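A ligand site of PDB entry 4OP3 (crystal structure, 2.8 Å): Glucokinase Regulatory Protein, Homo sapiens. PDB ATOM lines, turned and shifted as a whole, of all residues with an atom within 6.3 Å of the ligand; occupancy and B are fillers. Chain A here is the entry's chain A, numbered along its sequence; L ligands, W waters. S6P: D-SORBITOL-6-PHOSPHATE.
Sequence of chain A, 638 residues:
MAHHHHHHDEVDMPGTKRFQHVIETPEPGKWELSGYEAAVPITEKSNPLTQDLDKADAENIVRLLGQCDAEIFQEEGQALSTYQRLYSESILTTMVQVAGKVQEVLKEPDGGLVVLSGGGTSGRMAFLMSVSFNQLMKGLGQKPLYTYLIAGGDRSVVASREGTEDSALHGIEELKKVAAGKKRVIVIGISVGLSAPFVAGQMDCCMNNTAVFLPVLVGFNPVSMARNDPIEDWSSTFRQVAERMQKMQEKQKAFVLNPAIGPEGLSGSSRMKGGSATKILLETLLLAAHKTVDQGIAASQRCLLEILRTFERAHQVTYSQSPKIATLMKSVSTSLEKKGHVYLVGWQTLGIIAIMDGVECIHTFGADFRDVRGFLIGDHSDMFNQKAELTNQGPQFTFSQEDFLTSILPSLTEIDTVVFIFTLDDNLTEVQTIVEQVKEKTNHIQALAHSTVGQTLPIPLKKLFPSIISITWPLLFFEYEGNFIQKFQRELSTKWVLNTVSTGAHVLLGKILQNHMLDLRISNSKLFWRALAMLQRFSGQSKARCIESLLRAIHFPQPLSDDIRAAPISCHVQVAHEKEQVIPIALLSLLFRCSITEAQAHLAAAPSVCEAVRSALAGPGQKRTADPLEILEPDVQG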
ATOM      1  N   THR A  43      36.839  12.409 -12.650  1.00  0.00           N
ATOM      2  CA  THR A  43      35.525  13.046 -12.635  1.00  0.00           C
ATOM      3  C   THR A  43      34.909  13.147 -11.245  1.00  0.00           C
ATOM      4  O   THR A  43      34.202  14.084 -10.974  1.00  0.00           O
ATOM      5  CB  THR A  43      34.533  12.316 -13.552  1.00  0.00           C
ATOM      6  OG1 THR A  43      34.338  10.941 -13.145  1.00  0.00           O
ATOM      7  CG2 THR A  43      35.007  12.388 -14.988  1.00  0.00           C
ATOM      8  N   GLY A 118      23.925  10.185 -25.102  1.00  0.00           N
ATOM      9  CA  GLY A 118      24.424  10.452 -23.763  1.00  0.00           C
ATOM     10  C   GLY A 118      23.285  10.550 -22.783  1.00  0.00           C
ATOM     11  O   GLY A 118      22.159  10.863 -23.173  1.00  0.00           O
ATOM     12  N   GLY A 119      23.562  10.282 -21.514  1.00  0.00           N
ATOM     13  CA  GLY A 119      22.550  10.434 -20.442  1.00  0.00           C
ATOM     14  C   GLY A 119      22.690  11.851 -19.946  1.00  0.00           C
ATOM     15  O   GLY A 119      23.765  12.410 -20.086  1.00  0.00           O
ATOM     16  N   GLY A 120      21.651  12.435 -19.396  1.00  0.00           N
ATOM     17  CA  GLY A 120      21.782  13.695 -18.654  1.00  0.00           C
ATOM     18  C   GLY A 120      22.367  14.824 -19.509  1.00  0.00           C
ATOM     19  O   GLY A 120      22.088  14.949 -20.738  1.00  0.00           O
ATOM     20  N   THR A 121      23.232  15.632 -18.874  1.00  0.00           N
ATOM     21  CA  THR A 121      23.843  16.723 -19.558  1.00  0.00           C
ATOM     22  C   THR A 121      24.557  16.249 -20.815  1.00  0.00           C
ATOM     23  O   THR A 121      24.623  16.977 -21.804  1.00  0.00           O
ATOM     24  CB  THR A 121      24.788  17.511 -18.664  1.00  0.00           C
ATOM     25  OG1 THR A 121      24.090  18.022 -17.497  1.00  0.00           O
ATOM     26  CG2 THR A 121      25.362  18.674 -19.428  1.00  0.00           C
ATOM     27  N   SER A 122      25.094  15.022 -20.816  1.00  0.00           N
ATOM     28  CA  SER A 122      25.739  14.521 -22.037  1.00  0.00           C
ATOM     29  C   SER A 122      24.723  14.494 -23.147  1.00  0.00           C
ATOM     30  O   SER A 122      24.997  14.923 -24.258  1.00  0.00           O
ATOM     31  CB  SER A 122      26.318  13.136 -21.856  1.00  0.00           C
ATOM     32  OG  SER A 122      27.414  13.173 -20.981  1.00  0.00           O
ATOM     33  N   ARG A 124      21.905  16.233 -23.243  1.00  0.00           N
ATOM     34  CA  ARG A 124      21.562  17.594 -23.570  1.00  0.00           C
ATOM     35  C   ARG A 124      22.561  18.210 -24.570  1.00  0.00           C
ATOM     36  O   ARG A 124      22.174  18.767 -25.604  1.00  0.00           O
ATOM     37  CB  ARG A 124      21.479  18.426 -22.320  1.00  0.00           C
ATOM     38  CG  ARG A 124      20.355  17.987 -21.406  1.00  0.00           C
ATOM     39  CD  ARG A 124      20.105  19.019 -20.342  1.00  0.00           C
ATOM     40  NE  ARG A 124      20.120  18.486 -18.981  1.00  0.00           N
ATOM     41  CZ  ARG A 124      19.153  17.739 -18.438  1.00  0.00           C
ATOM     42  NH1 ARG A 124      18.102  17.405 -19.158  1.00  0.00           N
ATOM     43  NH2 ARG A 124      19.232  17.337 -17.184  1.00  0.00           N
ATOM     44  N   GLU A 162      17.259  11.604 -13.817  1.00  0.00           N
ATOM     45  CA  GLU A 162      18.540  10.926 -13.509  1.00  0.00           C
ATOM     46  C   GLU A 162      18.504   9.390 -13.567  1.00  0.00           C
ATOM     47  O   GLU A 162      19.524   8.771 -13.896  1.00  0.00           O
ATOM     48  CB  GLU A 162      19.016  11.318 -12.114  1.00  0.00           C
ATOM     49  CG  GLU A 162      19.370  12.780 -11.946  1.00  0.00           C
ATOM     50  CD  GLU A 162      20.644  13.138 -12.685  1.00  0.00           C
ATOM     51  OE1 GLU A 162      21.711  13.257 -12.033  1.00  0.00           O
ATOM     52  OE2 GLU A 162      20.555  13.257 -13.924  1.00  0.00           O
ATOM     53  N   GLU A 165      19.527   6.648 -16.970  1.00  0.00           N
ATOM     54  CA  GLU A 165      20.823   6.214 -17.540  1.00  0.00           C
ATOM     55  C   GLU A 165      21.322   4.755 -17.223  1.00  0.00           C
ATOM     56  O   GLU A 165      22.384   4.311 -17.734  1.00  0.00           O
ATOM     57  CB  GLU A 165      21.910   7.224 -17.145  1.00  0.00           C
ATOM     58  CG  GLU A 165      22.413   7.114 -15.723  1.00  0.00           C
ATOM     59  CD  GLU A 165      23.465   8.184 -15.376  1.00  0.00           C
ATOM     60  OE1 GLU A 165      23.098   9.365 -15.250  1.00  0.00           O
ATOM     61  OE2 GLU A 165      24.665   7.819 -15.199  1.00  0.00           O
ATOM     62  N   ILE A 190      28.638   9.640 -25.346  1.00  0.00           N
ATOM     63  CA  ILE A 190      29.263  10.598 -24.484  1.00  0.00           C
ATOM     64  C   ILE A 190      28.962  10.266 -23.027  1.00  0.00           C
ATOM     65  O   ILE A 190      27.829  10.425 -22.550  1.00  0.00           O
ATOM     66  CB  ILE A 190      28.720  12.005 -24.818  1.00  0.00           C
ATOM     67  CG1 ILE A 190      28.857  12.297 -26.321  1.00  0.00           C
ATOM     68  CG2 ILE A 190      29.418  13.080 -23.991  1.00  0.00           C
ATOM     69  CD1 ILE A 190      28.116  13.544 -26.733  1.00  0.00           C
ATOM     70  N   SER A 191      29.970   9.784 -22.317  1.00  0.00           N
ATOM     71  CA  SER A 191      29.840   9.617 -20.877  1.00  0.00           C
ATOM     72  C   SER A 191      31.060  10.279 -20.223  1.00  0.00           C
ATOM     73  O   SER A 191      32.207   9.807 -20.350  1.00  0.00           O
ATOM     74  CB  SER A 191      29.681   8.143 -20.456  1.00  0.00           C
ATOM     75  OG  SER A 191      29.295   8.001 -19.088  1.00  0.00           O
ATOM     76  N   VAL A 192      30.801  11.373 -19.529  1.00  0.00           N
ATOM     77  CA  VAL A 192      31.861  12.142 -19.013  1.00  0.00           C
ATOM     78  C   VAL A 192      32.711  11.277 -18.137  1.00  0.00           C
ATOM     79  O   VAL A 192      33.933  11.293 -18.256  1.00  0.00           O
ATOM     80  CB  VAL A 192      31.349  13.322 -18.230  1.00  0.00           C
ATOM     81  CG1 VAL A 192      32.487  13.895 -17.364  1.00  0.00           C
ATOM     82  CG2 VAL A 192      30.819  14.338 -19.214  1.00  0.00           C
ATOM     83  N   GLY A 193      32.052  10.513 -17.274  1.00  0.00           N
ATOM     84  CA  GLY A 193      32.770   9.655 -16.346  1.00  0.00           C
ATOM     85  C   GLY A 193      33.080   8.273 -16.865  1.00  0.00           C
ATOM     86  O   GLY A 193      33.509   7.464 -16.092  1.00  0.00           O
ATOM     87  N   LEU A 194      32.928   8.019 -18.166  1.00  0.00           N
ATOM     88  CA  LEU A 194      32.972   6.690 -18.720  1.00  0.00           C
ATOM     89  C   LEU A 194      32.197   5.783 -17.774  1.00  0.00           C
ATOM     90  O   LEU A 194      32.737   4.831 -17.166  1.00  0.00           O
ATOM     91  CB  LEU A 194      34.423   6.254 -18.888  1.00  0.00           C
ATOM     92  CG  LEU A 194      35.374   7.127 -19.722  1.00  0.00           C
ATOM     93  CD1 LEU A 194      36.649   6.357 -20.069  1.00  0.00           C
ATOM     94  CD2 LEU A 194      34.727   7.581 -21.012  1.00  0.00           C
ATOM     95  N   SER A 195      30.916   6.093 -17.643  1.00  0.00           N
ATOM     96  CA  SER A 195      30.101   5.576 -16.561  1.00  0.00           C
ATOM     97  C   SER A 195      28.734   5.051 -17.004  1.00  0.00           C
ATOM     98  O   SER A 195      28.309   4.045 -16.486  1.00  0.00           O
ATOM     99  CB  SER A 195      29.866   6.691 -15.522  1.00  0.00           C
ATOM    100  OG  SER A 195      28.612   6.539 -14.848  1.00  0.00           O
ATOM    101  N   ALA A 196      28.027   5.737 -17.888  1.00  0.00           N
ATOM    102  CA  ALA A 196      26.599   5.490 -18.029  1.00  0.00           C
ATOM    103  C   ALA A 196      26.384   4.186 -18.804  1.00  0.00           C
ATOM    104  O   ALA A 196      26.865   4.057 -19.907  1.00  0.00           O
ATOM    105  CB  ALA A 196      25.922   6.648 -18.717  1.00  0.00           C
ATOM    106  N   VAL A 199      25.251   4.361 -22.383  1.00  0.00           N
ATOM    107  CA  VAL A 199      26.233   4.477 -23.435  1.00  0.00           C
ATOM    108  C   VAL A 199      26.915   3.161 -23.614  1.00  0.00           C
ATOM    109  O   VAL A 199      27.071   2.678 -24.730  1.00  0.00           O
ATOM    110  CB  VAL A 199      27.277   5.602 -23.181  1.00  0.00           C
ATOM    111  CG1 VAL A 199      28.495   5.464 -24.075  1.00  0.00           C
ATOM    112  CG2 VAL A 199      26.651   6.986 -23.398  1.00  0.00           C
ATOM    113  N   GLY A 268      31.999  15.864  -8.872  1.00  0.00           N
ATOM    114  CA  GLY A 268      31.058  15.002  -9.522  1.00  0.00           C
ATOM    115  C   GLY A 268      29.941  15.689 -10.269  1.00  0.00           C
ATOM    116  O   GLY A 268      28.999  15.035 -10.730  1.00  0.00           O
ATOM    117  N   SER A 269      30.041  17.002 -10.437  1.00  0.00           N
ATOM    118  CA  SER A 269      29.003  17.740 -11.105  1.00  0.00           C
ATOM    119  C   SER A 269      29.465  17.922 -12.544  1.00  0.00           C
ATOM    120  O   SER A 269      29.985  18.977 -12.915  1.00  0.00           O
ATOM    121  CB  SER A 269      28.727  19.073 -10.397  1.00  0.00           C
ATOM    122  OG  SER A 269      27.495  19.654 -10.856  1.00  0.00           O
ATOM    123  N   SER A 270      29.272  16.871 -13.340  1.00  0.00           N
ATOM    124  CA  SER A 270      29.850  16.812 -14.649  1.00  0.00           C
ATOM    125  C   SER A 270      29.043  17.650 -15.672  1.00  0.00           C
ATOM    126  O   SER A 270      29.467  17.872 -16.838  1.00  0.00           O
ATOM    127  CB  SER A 270      30.085  15.339 -15.078  1.00  0.00           C
ATOM    128  OG  SER A 270      28.906  14.655 -15.492  1.00  0.00           O
ATOM    129  N   ARG A 271      27.896  18.163 -15.254  1.00  0.00           N
ATOM    130  CA  ARG A 271      27.183  19.108 -16.117  1.00  0.00           C
ATOM    131  C   ARG A 271      28.115  20.320 -16.438  1.00  0.00           C
ATOM    132  O   ARG A 271      28.022  20.872 -17.522  1.00  0.00           O
ATOM    133  CB  ARG A 271      25.859  19.575 -15.471  1.00  0.00           C
ATOM    134  CG  ARG A 271      26.020  20.667 -14.414  1.00  0.00           C
ATOM    135  CD  ARG A 271      24.826  20.795 -13.486  1.00  0.00           C
ATOM    136  NE  ARG A 271      24.826  22.056 -12.748  1.00  0.00           N
ATOM    137  CZ  ARG A 271      24.224  23.183 -13.165  1.00  0.00           C
ATOM    138  NH1 ARG A 271      23.584  23.206 -14.322  1.00  0.00           N
ATOM    139  NH2 ARG A 271      24.298  24.288 -12.417  1.00  0.00           N
ATOM    140  N   MET A 272      29.003  20.701 -15.515  1.00  0.00           N
ATOM    141  CA  MET A 272      29.887  21.859 -15.669  1.00  0.00           C
ATOM    142  C   MET A 272      31.046  21.621 -16.630  1.00  0.00           C
ATOM    143  O   MET A 272      30.814  21.547 -17.840  1.00  0.00           O
ATOM    144  CB  MET A 272      30.371  22.353 -14.284  1.00  0.00           C
ATOM    145  CG  MET A 272      29.246  22.934 -13.455  1.00  0.00           C
ATOM    146  SD  MET A 272      29.789  23.193 -11.779  1.00  0.00           S
ATOM    147  CE  MET A 272      29.963  24.977 -11.831  1.00  0.00           C
ATOM    148  N   GLU A 360      18.557  21.455 -14.353  1.00  0.00           N
ATOM    149  CA  GLU A 360      19.674  20.735 -13.725  1.00  0.00           C
ATOM    150  C   GLU A 360      19.818  21.109 -12.277  1.00  0.00           C
ATOM    151  O   GLU A 360      20.377  20.339 -11.489  1.00  0.00           O
ATOM    152  CB  GLU A 360      20.976  20.966 -14.479  1.00  0.00           C
ATOM    153  CG  GLU A 360      21.030  20.196 -15.791  1.00  0.00           C
ATOM    154  CD  GLU A 360      22.116  20.694 -16.732  1.00  0.00           C
ATOM    155  OE1 GLU A 360      22.927  21.528 -16.257  1.00  0.00           O
ATOM    156  OE2 GLU A 360      22.153  20.257 -17.919  1.00  0.00           O
ATOM    157  N   HIS A 363      17.958  18.241  -9.634  1.00  0.00           N
ATOM    158  CA  HIS A 363      18.697  17.110  -9.141  1.00  0.00           C
ATOM    159  C   HIS A 363      19.967  17.565  -8.492  1.00  0.00           C
ATOM    160  O   HIS A 363      20.336  17.067  -7.460  1.00  0.00           O
ATOM    161  CB  HIS A 363      18.910  16.025 -10.203  1.00  0.00           C
ATOM    162  CG  HIS A 363      19.590  16.453 -11.461  1.00  0.00           C
ATOM    163  ND1 HIS A 363      18.938  16.469 -12.678  1.00  0.00           N
ATOM    164  CD2 HIS A 363      20.881  16.755 -11.747  1.00  0.00           C
ATOM    165  CE1 HIS A 363      19.775  16.809 -13.635  1.00  0.00           C
ATOM    166  NE2 HIS A 363      20.967  16.984 -13.093  1.00  0.00           N
ATOM    167  N   THR A 364      20.645  18.563  -9.054  1.00  0.00           N
ATOM    168  CA  THR A 364      21.933  18.965  -8.510  1.00  0.00           C
ATOM    169  C   THR A 364      21.813  19.605  -7.123  1.00  0.00           C
ATOM    170  O   THR A 364      22.664  19.375  -6.280  1.00  0.00           O
ATOM    171  CB  THR A 364      22.711  19.846  -9.512  1.00  0.00           C
ATOM    172  OG1 THR A 364      22.836  19.170 -10.784  1.00  0.00           O
ATOM    173  CG2 THR A 364      24.095  20.165  -8.965  1.00  0.00           C
ATOM    174  N   ASN A 524      20.212   7.311  -9.221  1.00  0.00           N
ATOM    175  CA  ASN A 524      20.769   6.270 -10.104  1.00  0.00           C
ATOM    176  C   ASN A 524      21.939   5.610  -9.409  1.00  0.00           C
ATOM    177  O   ASN A 524      22.323   6.003  -8.311  1.00  0.00           O
ATOM    178  CB  ASN A 524      21.162   6.816 -11.493  1.00  0.00           C
ATOM    179  CG  ASN A 524      22.142   7.989 -11.448  1.00  0.00           C
ATOM    180  OD1 ASN A 524      21.989   8.997 -12.182  1.00  0.00           O
ATOM    181  ND2 ASN A 524      23.168   7.863 -10.627  1.00  0.00           N
ATOM    182  N   LYS A 526      25.225   5.490 -10.095  1.00  0.00           N
ATOM    183  CA  LYS A 526      26.380   6.375  -9.891  1.00  0.00           C
ATOM    184  C   LYS A 526      26.280   7.247  -8.644  1.00  0.00           C
ATOM    185  O   LYS A 526      27.287   7.469  -7.954  1.00  0.00           O
ATOM    186  CB  LYS A 526      26.593   7.258 -11.103  1.00  0.00           C
ATOM    187  CG  LYS A 526      27.729   8.276 -10.942  1.00  0.00           C
ATOM    188  CD  LYS A 526      28.050   8.982 -12.255  1.00  0.00           C
ATOM    189  CE  LYS A 526      26.972   9.964 -12.686  1.00  0.00           C
ATOM    190  NZ  LYS A 526      26.995  10.105 -14.160  1.00  0.00           N
ATOM    191  N   ARG A 530      28.436   7.424  -5.171  1.00  0.00           N
ATOM    192  CA  ARG A 530      28.989   8.714  -4.753  1.00  0.00           C
ATOM    193  C   ARG A 530      28.537   9.007  -3.335  1.00  0.00           C
ATOM    194  O   ARG A 530      29.324   9.528  -2.528  1.00  0.00           O
ATOM    195  CB  ARG A 530      28.545   9.815  -5.715  1.00  0.00           C
ATOM    196  CG  ARG A 530      28.953  11.238  -5.333  1.00  0.00           C
ATOM    197  CD  ARG A 530      28.538  12.246  -6.384  1.00  0.00           C
ATOM    198  NE  ARG A 530      28.954  11.877  -7.747  1.00  0.00           N
ATOM    199  CZ  ARG A 530      28.392  12.346  -8.867  1.00  0.00           C
ATOM    200  NH1 ARG A 530      27.368  13.193  -8.829  1.00  0.00           N
ATOM    201  NH2 ARG A 530      28.836  11.958 -10.049  1.00  0.00           N
HETATM  202  C1  S6P L   1      25.909  15.962 -13.978  1.00  0.00           C
HETATM  203  C2  S6P L   1      24.463  15.656 -14.318  1.00  0.00           C
HETATM  204  C3  S6P L   1      24.276  14.167 -14.508  1.00  0.00           C
HETATM  205  C4  S6P L   1      25.151  13.696 -15.624  1.00  0.00           C
HETATM  206  C5  S6P L   1      24.644  12.352 -16.105  1.00  0.00           C
HETATM  207  C6  S6P L   1      25.521  11.812 -17.234  1.00  0.00           C
HETATM  208  O1  S6P L   1      25.806  16.810 -12.858  1.00  0.00           O
HETATM  209  O2  S6P L   1      23.646  16.134 -13.246  1.00  0.00           O
HETATM  210  O3  S6P L   1      22.952  13.916 -14.938  1.00  0.00           O
HETATM  211  O4  S6P L   1      25.051  14.629 -16.714  1.00  0.00           O
HETATM  212  O5  S6P L   1      24.653  11.462 -14.989  1.00  0.00           O
HETATM  213  O6  S6P L   1      26.702  11.291 -16.668  1.00  0.00           O
HETATM  214  P   S6P L   1      28.015  11.027 -17.518  1.00  0.00           P
HETATM  215  O1P S6P L   1      29.177  10.913 -16.566  1.00  0.00           O
HETATM  216  O2P S6P L   1      27.760   9.770 -18.468  1.00  0.00           O
HETATM  217  O3P S6P L   1      28.248  12.357 -18.455  1.00  0.00           O
HETATM  218  O   HOH W   1      23.607  11.244 -12.671  1.00  0.00           O
HETATM  219  O   HOH W   2      27.115   8.281 -16.068  1.00  0.00           O
HETATM  220  O   HOH W   3      25.182  18.175 -10.781  1.00  0.00           O
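The side-chain hydroxyl of Ser 191 lies within hydrogen-bond range of an oxygen (O2P) of the ligand.
OE1 of Glu 165 lies within hydrogen-bond range of O5 of the ligand (2.6 Å).
The side-chain carboxylate (OE2) of Glu 162 sits at hydrogen-bond distance from an oxygen (O3) of the ligand (2.7 Å).
OG of Ser 122 sits at hydrogen-bond distance from O3P of the ligand (2.8 Å).
NZ of Lys 526 lies within salt-bridge range of O1P of the ligand (3.3 Å).
O2 of the ligand sits at hydrogen-bond distance from NE2 of His 363 (2.8 Å).
The backbone NH (N) of Val 192 is in hydrogen-bond range of an oxygen (O3P) of the ligand, 2.9 Å away.
N of Gly 193 lies within hydrogen-bond range of O1P of the ligand, at 3.0 Å.
The backbone NH of Thr 121 sits at hydrogen-bond distance from an oxygen (O4) of the ligand (3.0 Å).
The backbone NH (N) of Arg 271 sits close to an oxygen (O1) of the ligand, 3.5 Å away.
N of Ser 270 lies within hydrogen-bond range of O1 of the ligand (3.5 Å).
The side-chain hydroxyl (OG) of Ser 191 lies within hydrogen-bond range of the backbone NH (N) of Ala 196 (2.9 Å).
N of Ser 195 lies within hydrogen-bond range of OG of Ser 191.
OE1 of Glu 165 sits close to OD1 of Asn 524, 3.3 Å away.
The backbone carbonyl oxygen of Glu 162 lies close to the side-chain amide oxygen of Asn 524, 3.0 Å away.
The backbone NH of Lys 526 sits close to the side-chain amide nitrogen of Asn 524 (3.2 Å).
The side-chain hydroxyl of Thr 121 sits at hydrogen-bond distance from the side-chain carboxylate of Glu 360 (3.0 Å).
The guanidinium group (NH1) of Arg 271 is in salt-bridge range of the side-chain carboxylate (OE1) of Glu 360 (2.6 Å).
The side-chain hydroxyl (OG1) of Thr 364 lies within hydrogen-bond range of the backbone carbonyl oxygen (O) of Glu 360, at 2.8 Å.
Water W3 lies within hydrogen-bond range of the side-chain hydroxyl (OG1) of Thr 364 (2.5 Å), an oxygen (O1) of the ligand (2.6 Å) and the side-chain hydroxyl (OG) of Ser 269 (2.7 Å).
Water W2 lies within hydrogen-bond range of OG of Ser 195 (2.6 Å), OE2 of Glu 165 (2.6 Å), NZ of Lys 526 (2.6 Å), O2P of the ligand (2.9 Å) and N of Ala 196 (3.3 Å).
O of Gly 119 touches C6 of the ligand, at 3.4 Å.
C of Gly 120 touches O4 of the ligand, at 3.9 Å.
Ala 196 touches the ligand (CB to O2P, 3.6 Å).
Ser 269 touches the ligand (CA to O1, 3.8 Å).
Thr 364 touches the ligand.
Hydrophobic or aromatic side chains that line the ligand: Val 192, Ala 196 and His 363.
The nearest printed residue that does not touch the ligand is Ile 190 (4.1 Å).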
